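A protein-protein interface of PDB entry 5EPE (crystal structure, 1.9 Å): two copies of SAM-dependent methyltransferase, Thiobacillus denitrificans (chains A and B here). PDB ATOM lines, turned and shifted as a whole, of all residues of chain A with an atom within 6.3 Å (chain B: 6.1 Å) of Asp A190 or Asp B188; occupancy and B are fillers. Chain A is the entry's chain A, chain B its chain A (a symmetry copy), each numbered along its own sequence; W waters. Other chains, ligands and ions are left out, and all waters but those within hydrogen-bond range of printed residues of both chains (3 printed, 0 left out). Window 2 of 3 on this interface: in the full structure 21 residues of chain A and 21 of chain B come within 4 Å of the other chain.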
ATOM      1  N   THR A  21       7.939  23.102  31.062  1.00  0.00           N
ATOM      2  CA  THR A  21       8.547  24.408  31.149  1.00  0.00           C
ATOM      3  C   THR A  21       8.177  25.116  32.445  1.00  0.00           C
ATOM      4  O   THR A  21       7.258  24.698  33.135  1.00  0.00           O
ATOM      5  CB  THR A  21       8.051  25.275  30.000  1.00  0.00           C
ATOM      6  OG1 THR A  21       6.611  25.355  29.995  1.00  0.00           O
ATOM      7  CG2 THR A  21       8.555  24.747  28.678  1.00  0.00           C
ATOM      8  N   ASP A 188       4.008  19.476  25.865  1.00  0.00           N
ATOM      9  CA  ASP A 188       3.959  19.524  24.417  1.00  0.00           C
ATOM     10  C   ASP A 188       5.373  19.274  23.916  1.00  0.00           C
ATOM     11  O   ASP A 188       6.288  19.080  24.732  1.00  0.00           O
ATOM     12  CB  ASP A 188       3.399  20.818  23.933  1.00  0.00           C
ATOM     13  CG  ASP A 188       4.259  22.043  24.283  1.00  0.00           C
ATOM     14  OD1 ASP A 188       5.310  22.029  24.954  1.00  0.00           O
ATOM     15  OD2 ASP A 188       3.750  23.138  23.951  1.00  0.00           O
ATOM     16  N   GLN A 189       5.555  19.272  22.602  1.00  0.00           N
ATOM     17  CA  GLN A 189       6.882  18.982  22.075  1.00  0.00           C
ATOM     18  C   GLN A 189       7.941  19.994  22.507  1.00  0.00           C
ATOM     19  O   GLN A 189       9.084  19.588  22.749  1.00  0.00           O
ATOM     20  CB  GLN A 189       6.860  18.807  20.586  1.00  0.00           C
ATOM     21  CG  GLN A 189       6.058  17.582  20.186  1.00  0.00           C
ATOM     22  CD  GLN A 189       5.837  17.491  18.681  1.00  0.00           C
ATOM     23  OE1 GLN A 189       5.466  18.489  18.003  1.00  0.00           O
ATOM     24  NE2 GLN A 189       6.165  16.328  18.109  1.00  0.00           N
ATOM     25  N   ASP A 190       7.563  21.264  22.658  1.00  0.00           N
ATOM     26  CA  ASP A 190       8.465  22.293  23.129  1.00  0.00           C
ATOM     27  C   ASP A 190       8.943  22.083  24.539  1.00  0.00           C
ATOM     28  O   ASP A 190      10.101  22.324  24.856  1.00  0.00           O
ATOM     29  CB  ASP A 190       7.865  23.676  22.968  1.00  0.00           C
ATOM     30  CG  ASP A 190       7.695  24.062  21.474  1.00  0.00           C
ATOM     31  OD1 ASP A 190       8.539  23.762  20.572  1.00  0.00           O
ATOM     32  OD2 ASP A 190       6.652  24.695  21.186  1.00  0.00           O
ATOM     33  N   SER A 191       8.077  21.554  25.404  1.00  0.00           N
ATOM     34  CA  SER A 191       8.491  21.280  26.760  1.00  0.00           C
ATOM     35  C   SER A 191       9.381  20.054  26.850  1.00  0.00           C
ATOM     36  O   SER A 191      10.327  20.047  27.648  1.00  0.00           O
ATOM     37  CB  SER A 191       7.292  21.334  27.743  1.00  0.00           C
ATOM     38  OG  SER A 191       6.462  20.303  27.579  1.00  0.00           O
ATOM     39  N   TRP A 192       9.143  19.059  26.016  1.00  0.00           N
ATOM     40  CA  TRP A 192      10.056  17.953  25.884  1.00  0.00           C
ATOM     41  C   TRP A 192      11.440  18.432  25.409  1.00  0.00           C
ATOM     42  O   TRP A 192      12.453  17.955  25.907  1.00  0.00           O
ATOM     43  CB  TRP A 192       9.530  16.900  24.900  1.00  0.00           C
ATOM     44  CG  TRP A 192       8.717  15.782  25.513  1.00  0.00           C
ATOM     45  CD1 TRP A 192       7.386  15.589  25.418  1.00  0.00           C
ATOM     46  CD2 TRP A 192       9.222  14.711  26.296  1.00  0.00           C
ATOM     47  NE1 TRP A 192       7.002  14.475  26.120  1.00  0.00           N
ATOM     48  CE2 TRP A 192       8.125  13.909  26.663  1.00  0.00           C
ATOM     49  CE3 TRP A 192      10.500  14.357  26.734  1.00  0.00           C
ATOM     50  CZ2 TRP A 192       8.279  12.760  27.408  1.00  0.00           C
ATOM     51  CZ3 TRP A 192      10.642  13.229  27.485  1.00  0.00           C
ATOM     52  CH2 TRP A 192       9.535  12.463  27.850  1.00  0.00           C
ATOM     53  N   ASP A 193      11.457  19.347  24.453  1.00  0.00           N
ATOM     54  CA  ASP A 193      12.735  19.904  23.950  1.00  0.00           C
ATOM     55  C   ASP A 193      13.526  20.526  25.070  1.00  0.00           C
ATOM     56  O   ASP A 193      14.747  20.326  25.149  1.00  0.00           O
ATOM     57  CB  ASP A 193      12.519  20.971  22.870  1.00  0.00           C
ATOM     58  CG  ASP A 193      12.045  20.425  21.555  1.00  0.00           C
ATOM     59  OD1 ASP A 193      12.008  19.190  21.317  1.00  0.00           O
ATOM     60  OD2 ASP A 193      11.536  21.227  20.716  1.00  0.00           O
ATOM     61  N   ARG A 194      12.832  21.293  25.944  1.00  0.00           N
ATOM     62  CA  ARG A 194      13.498  21.921  27.106  1.00  0.00           C
ATOM     63  C   ARG A 194      14.166  20.937  28.030  1.00  0.00           C
ATOM     64  O   ARG A 194      15.325  21.167  28.443  1.00  0.00           O
ATOM     65  CB  ARG A 194      12.585  22.821  27.971  1.00  0.00           C
ATOM     66  CG  ARG A 194      11.985  24.042  27.286  1.00  0.00           C
ATOM     67  CD  ARG A 194      12.994  25.134  26.984  1.00  0.00           C
ATOM     68  NE  ARG A 194      13.687  24.747  25.748  1.00  0.00           N
ATOM     69  CZ  ARG A 194      14.998  24.513  25.608  1.00  0.00           C
ATOM     70  NH1 ARG A 194      15.438  24.086  24.414  1.00  0.00           N
ATOM     71  NH2 ARG A 194      15.861  24.626  26.632  1.00  0.00           N
ATOM     72  N   TYR A 195      13.460  19.867  28.365  1.00  0.00           N
ATOM     73  CA  TYR A 195      13.991  18.828  29.199  1.00  0.00           C
ATOM     74  C   TYR A 195      15.202  18.071  28.555  1.00  0.00           C
ATOM     75  O   TYR A 195      16.250  17.900  29.208  1.00  0.00           O
ATOM     76  CB  TYR A 195      12.874  17.851  29.599  1.00  0.00           C
ATOM     77  CG  TYR A 195      13.364  16.663  30.333  1.00  0.00           C
ATOM     78  CD1 TYR A 195      14.019  16.822  31.555  1.00  0.00           C
ATOM     79  CD2 TYR A 195      13.243  15.400  29.794  1.00  0.00           C
ATOM     80  CE1 TYR A 195      14.503  15.761  32.235  1.00  0.00           C
ATOM     81  CE2 TYR A 195      13.740  14.322  30.449  1.00  0.00           C
ATOM     82  CZ  TYR A 195      14.372  14.523  31.666  1.00  0.00           C
ATOM     83  OH  TYR A 195      14.901  13.469  32.316  1.00  0.00           O
ATOM     84  N   TYR A 230      16.252  11.145  20.245  1.00  0.00           N
ATOM     85  CA  TYR A 230      15.154  11.943  20.795  1.00  0.00           C
ATOM     86  C   TYR A 230      14.156  12.362  19.683  1.00  0.00           C
ATOM     87  O   TYR A 230      12.956  12.188  19.825  1.00  0.00           O
ATOM     88  CB  TYR A 230      15.720  13.183  21.552  1.00  0.00           C
ATOM     89  CG  TYR A 230      14.683  14.195  21.812  1.00  0.00           C
ATOM     90  CD1 TYR A 230      13.683  13.942  22.739  1.00  0.00           C
ATOM     91  CD2 TYR A 230      14.654  15.393  21.102  1.00  0.00           C
ATOM     92  CE1 TYR A 230      12.666  14.838  22.939  1.00  0.00           C
ATOM     93  CE2 TYR A 230      13.663  16.324  21.322  1.00  0.00           C
ATOM     94  CZ  TYR A 230      12.670  16.062  22.266  1.00  0.00           C
ATOM     95  OH  TYR A 230      11.625  16.940  22.493  1.00  0.00           O
ATOM     96  N   ARG A 235      10.215  12.556  20.625  1.00  0.00           N
ATOM     97  CA  ARG A 235       9.515  13.806  20.317  1.00  0.00           C
ATOM     98  C   ARG A 235       8.152  13.576  19.674  1.00  0.00           C
ATOM     99  O   ARG A 235       7.213  14.292  19.933  1.00  0.00           O
ATOM    100  CB  ARG A 235      10.398  14.704  19.451  1.00  0.00           C
ATOM    101  CG  ARG A 235       9.944  16.133  19.417  1.00  0.00           C
ATOM    102  CD  ARG A 235      10.898  17.017  18.631  1.00  0.00           C
ATOM    103  NE  ARG A 235      10.638  18.418  18.938  1.00  0.00           N
ATOM    104  CZ  ARG A 235       9.725  19.176  18.339  1.00  0.00           C
ATOM    105  NH1 ARG A 235       9.057  18.744  17.323  1.00  0.00           N
ATOM    106  NH2 ARG A 235       9.496  20.446  18.796  1.00  0.00           N
ATOM    107  N   PRO B  19       9.651  32.642  12.153  1.00  0.00           N
ATOM    108  CA  PRO B  19       8.530  32.016  12.934  1.00  0.00           C
ATOM    109  C   PRO B  19       8.869  31.704  14.403  1.00  0.00           C
ATOM    110  O   PRO B  19       8.850  30.564  14.857  1.00  0.00           O
ATOM    111  CB  PRO B  19       8.220  30.767  12.115  1.00  0.00           C
ATOM    112  CG  PRO B  19       9.529  30.410  11.436  1.00  0.00           C
ATOM    113  CD  PRO B  19      10.202  31.714  11.141  1.00  0.00           C
ATOM    114  N   THR B  21       8.110  33.414  18.372  1.00  0.00           N
ATOM    115  CA  THR B  21       7.486  34.400  19.221  1.00  0.00           C
ATOM    116  C   THR B  21       8.501  35.093  20.119  1.00  0.00           C
ATOM    117  O   THR B  21       9.624  34.627  20.254  1.00  0.00           O
ATOM    118  CB  THR B  21       6.469  33.719  20.127  1.00  0.00           C
ATOM    119  OG1 THR B  21       7.084  32.664  20.894  1.00  0.00           O
ATOM    120  CG2 THR B  21       5.314  33.179  19.318  1.00  0.00           C
ATOM    121  N   LYS B  24       9.524  32.398  22.571  1.00  0.00           N
ATOM    122  CA  LYS B  24      10.576  31.518  22.037  1.00  0.00           C
ATOM    123  C   LYS B  24      11.954  32.131  22.012  1.00  0.00           C
ATOM    124  O   LYS B  24      12.950  31.485  22.340  1.00  0.00           O
ATOM    125  CB  LYS B  24      10.210  31.013  20.675  1.00  0.00           C
ATOM    126  CG  LYS B  24       9.183  29.913  20.843  1.00  0.00           C
ATOM    127  CD  LYS B  24       8.739  29.269  19.599  1.00  0.00           C
ATOM    128  CE  LYS B  24       7.568  28.310  19.862  1.00  0.00           C
ATOM    129  NZ  LYS B  24       8.064  27.074  20.456  1.00  0.00           N
ATOM    130  N   VAL B 185      15.748  25.273  19.953  1.00  0.00           N
ATOM    131  CA  VAL B 185      14.415  25.816  20.248  1.00  0.00           C
ATOM    132  C   VAL B 185      13.703  25.869  18.895  1.00  0.00           C
ATOM    133  O   VAL B 185      14.152  26.527  17.970  1.00  0.00           O
ATOM    134  CB  VAL B 185      14.466  27.225  20.912  1.00  0.00           C
ATOM    135  CG1 VAL B 185      13.067  27.806  21.179  1.00  0.00           C
ATOM    136  CG2 VAL B 185      15.214  27.150  22.250  1.00  0.00           C
ATOM    137  N   LEU B 186      12.593  25.153  18.794  1.00  0.00           N
ATOM    138  CA  LEU B 186      11.896  25.017  17.547  1.00  0.00           C
ATOM    139  C   LEU B 186      10.634  25.853  17.494  1.00  0.00           C
ATOM    140  O   LEU B 186       9.988  26.044  18.515  1.00  0.00           O
ATOM    141  CB  LEU B 186      11.579  23.513  17.315  1.00  0.00           C
ATOM    142  CG  LEU B 186      12.785  22.547  17.353  1.00  0.00           C
ATOM    143  CD1 LEU B 186      12.367  21.161  16.840  1.00  0.00           C
ATOM    144  CD2 LEU B 186      13.983  23.001  16.641  1.00  0.00           C
ATOM    145  N   ALA B 187      10.279  26.335  16.296  1.00  0.00           N
ATOM    146  CA  ALA B 187       8.951  26.886  16.086  1.00  0.00           C
ATOM    147  C   ALA B 187       7.899  25.828  16.335  1.00  0.00           C
ATOM    148  O   ALA B 187       8.143  24.643  16.206  1.00  0.00           O
ATOM    149  CB  ALA B 187       8.804  27.417  14.664  1.00  0.00           C
ATOM    150  N   ASP B 188       6.717  26.278  16.714  1.00  0.00           N
ATOM    151  CA  ASP B 188       5.517  25.467  16.666  1.00  0.00           C
ATOM    152  C   ASP B 188       4.548  26.162  15.722  1.00  0.00           C
ATOM    153  O   ASP B 188       4.881  27.224  15.173  1.00  0.00           O
ATOM    154  CB  ASP B 188       4.944  25.258  18.025  1.00  0.00           C
ATOM    155  CG  ASP B 188       4.453  26.548  18.703  1.00  0.00           C
ATOM    156  OD1 ASP B 188       4.546  27.700  18.233  1.00  0.00           O
ATOM    157  OD2 ASP B 188       4.049  26.388  19.877  1.00  0.00           O
ATOM    158  N   GLN B 189       3.372  25.579  15.529  1.00  0.00           N
ATOM    159  CA  GLN B 189       2.433  26.179  14.591  1.00  0.00           C
ATOM    160  C   GLN B 189       1.991  27.585  14.992  1.00  0.00           C
ATOM    161  O   GLN B 189       1.813  28.426  14.102  1.00  0.00           O
ATOM    162  CB  GLN B 189       1.259  25.284  14.332  1.00  0.00           C
ATOM    163  CG  GLN B 189       1.683  24.009  13.623  1.00  0.00           C
ATOM    164  CD  GLN B 189       0.558  22.986  13.533  1.00  0.00           C
ATOM    165  OE1 GLN B 189      -0.165  22.705  14.528  1.00  0.00           O
ATOM    166  NE2 GLN B 189       0.312  22.490  12.316  1.00  0.00           N
ATOM    167  N   ASP B 190       1.873  27.853  16.294  1.00  0.00           N
ATOM    168  CA  ASP B 190       1.527  29.168  16.789  1.00  0.00           C
ATOM    169  C   ASP B 190       2.557  30.221  16.484  1.00  0.00           C
ATOM    170  O   ASP B 190       2.224  31.353  16.157  1.00  0.00           O
ATOM    171  CB  ASP B 190       1.214  29.139  18.272  1.00  0.00           C
ATOM    172  CG  ASP B 190      -0.081  28.337  18.572  1.00  0.00           C
ATOM    173  OD1 ASP B 190      -1.113  28.366  17.831  1.00  0.00           O
ATOM    174  OD2 ASP B 190      -0.059  27.629  19.607  1.00  0.00           O
ATOM    175  N   SER B 191       3.837  29.849  16.512  1.00  0.00           N
ATOM    176  CA  SER B 191       4.870  30.802  16.179  1.00  0.00           C
ATOM    177  C   SER B 191       4.944  31.066  14.687  1.00  0.00           C
ATOM    178  O   SER B 191       5.188  32.211  14.285  1.00  0.00           O
ATOM    179  CB  SER B 191       6.208  30.459  16.886  1.00  0.00           C
ATOM    180  OG  SER B 191       6.778  29.365  16.377  1.00  0.00           O
ATOM    181  N   TRP B 192       4.679  30.064  13.870  1.00  0.00           N
ATOM    182  CA  TRP B 192       4.520  30.269  12.454  1.00  0.00           C
ATOM    183  C   TRP B 192       3.349  31.225  12.162  1.00  0.00           C
ATOM    184  O   TRP B 192       3.465  32.083  11.294  1.00  0.00           O
ATOM    185  CB  TRP B 192       4.277  28.946  11.715  1.00  0.00           C
ATOM    186  CG  TRP B 192       5.515  28.258  11.184  1.00  0.00           C
ATOM    187  CD1 TRP B 192       6.094  27.136  11.654  1.00  0.00           C
ATOM    188  CD2 TRP B 192       6.289  28.671  10.067  1.00  0.00           C
ATOM    189  NE1 TRP B 192       7.213  26.820  10.925  1.00  0.00           N
ATOM    190  CE2 TRP B 192       7.347  27.752   9.930  1.00  0.00           C
ATOM    191  CE3 TRP B 192       6.197  29.741   9.174  1.00  0.00           C
ATOM    192  CZ2 TRP B 192       8.271  27.852   8.914  1.00  0.00           C
ATOM    193  CZ3 TRP B 192       7.125  29.841   8.181  1.00  0.00           C
ATOM    194  CH2 TRP B 192       8.174  28.927   8.081  1.00  0.00           C
ATOM    195  N   ASP B 193       2.248  31.052  12.875  1.00  0.00           N
ATOM    196  CA  ASP B 193       1.076  31.943  12.701  1.00  0.00           C
ATOM    197  C   ASP B 193       1.453  33.378  12.946  1.00  0.00           C
ATOM    198  O   ASP B 193       1.037  34.265  12.186  1.00  0.00           O
ATOM    199  CB  ASP B 193      -0.074  31.583  13.650  1.00  0.00           C
ATOM    200  CG  ASP B 193      -0.780  30.305  13.301  1.00  0.00           C
ATOM    201  OD1 ASP B 193      -0.561  29.691  12.224  1.00  0.00           O
ATOM    202  OD2 ASP B 193      -1.511  29.760  14.180  1.00  0.00           O
ATOM    203  N   TRP B 240      10.743  24.833  11.544  1.00  0.00           N
ATOM    204  CA  TRP B 240      11.797  25.847  11.666  1.00  0.00           C
ATOM    205  C   TRP B 240      12.337  25.805  13.095  1.00  0.00           C
ATOM    206  O   TRP B 240      11.630  25.443  14.072  1.00  0.00           O
ATOM    207  CB  TRP B 240      11.282  27.242  11.275  1.00  0.00           C
ATOM    208  CG  TRP B 240      12.345  28.239  11.022  1.00  0.00           C
ATOM    209  CD1 TRP B 240      12.934  28.548   9.815  1.00  0.00           C
ATOM    210  CD2 TRP B 240      12.923  29.124  11.986  1.00  0.00           C
ATOM    211  NE1 TRP B 240      13.902  29.489  10.002  1.00  0.00           N
ATOM    212  CE2 TRP B 240      13.875  29.905  11.313  1.00  0.00           C
ATOM    213  CE3 TRP B 240      12.711  29.334  13.366  1.00  0.00           C
ATOM    214  CZ2 TRP B 240      14.633  30.901  11.973  1.00  0.00           C
ATOM    215  CZ3 TRP B 240      13.461  30.277  14.041  1.00  0.00           C
ATOM    216  CH2 TRP B 240      14.412  31.059  13.347  1.00  0.00           C
HETATM  217  O   HOH W   1      11.352  23.826  21.076  1.00  0.00           O
HETATM  218  O   HOH W   2       7.783  22.720  18.110  1.00  0.00           O
HETATM  219  O   HOH W   3       2.630  25.887  22.720  1.00  0.00           O
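The side-chain carboxylate (OD1) of Asp A190 sits close to the backbone carbonyl oxygen (O) of Leu B186 (3.4 Å). The side-chain carboxylate of Asp B188 sits close to the side-chain carboxylate of Asp A190. OD2 of Asp A190 lies within salt-bridge range of NZ of Lys B24 (2.9 Å).
O of Tyr A230 is in hydrogen-bond range of N of Arg A235. The side-chain hydroxyl (OH) of Tyr A230 sits at hydrogen-bond distance from the side-chain carboxylate (OD1) of Asp A193, 2.6 Å away. The guanidinium group (NE) of Arg A235 lies within salt-bridge range of the side-chain carboxylate (OD1) of Asp A193, at 2.9 Å. The backbone carbonyl oxygen (O) of Arg A235 sits at hydrogen-bond distance from the side-chain amide nitrogen (NE2) of Gln A189. O of Leu B186 is in hydrogen-bond range of NZ of Lys B24, at 2.9 Å. The side-chain carboxylate of Asp B188 sits at hydrogen-bond distance from the backbone NH of Ser B191 (2.8 Å).
Leu B186 touches Asp A193. NH1 of Arg A194 touches CG2 of Val B185, at 3.8 Å. NH2 of Arg A235 touches CD1 of Leu B186, 3.5 Å away.
Asp A190 touches just these residues of chain B: Lys B24 (2.9 Å), Leu B186 (3.4 Å) and Asp B188 (3.4 Å). Asp B188 touches just one residue of chain A: Asp A190 (3.4 Å). Of the printed residues of chain B, Arg A194 touches Val B185 (3.8 Å). Printed residues of chain A within 4 Å of Leu B186: Asp A190, Asp A193 and Arg A235. Of the printed residues of chain A, Lys B24 touches Asp A190. Of the printed residues of chain B, Arg A235 touches Leu B186 (3.5 Å). Trp B192 touches none of the printed residues of chain A. The nearest residue of chain B that does not touch Asp A190 is Ala B187 (4.5 Å). The nearest residue of chain A that does not touch Asp B188 is Asp A188 (5.2 Å). The nearest printed residue of chain A that does not touch Val B185 is Asp A193 (5.4 Å).
Printed residues of chain B that touch a printed residue of chain A: Lys B24, Val B185, Leu B186 and Asp B188. Hydrophobic or aromatic side chains of chain B within 4 Å of the printed part of chain A: Val B185 and Leu B186. Among the printed residues, 6 pairs touch across the chains. Among the printed residues, Asp or Glu carboxylates within 4 Å of a Lys or Arg side-chain nitrogen of the other chain: Asp A190 with Lys B24.
Asp A190 touches Asp B188, but with the chains exchanged Asp A188 does not touch Asp B190 (7.3 Å).
Water W1 lies within hydrogen-bond range of OD2 of Asp A193 (2.6 Å), OD1 of Asp A190 (2.9 Å) and N of Leu B186 (2.9 Å). Water W2 lies within hydrogen-bond range of O of Ala B187 (2.7 Å), OD1 of Asp A190 (2.8 Å) and NH2 of Arg A235 (2.9 Å). Water W3 lies within hydrogen-bond range of OD2 of Asp A188 (3.2 Å) and OD2 of Asp B188 (3.2 Å).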
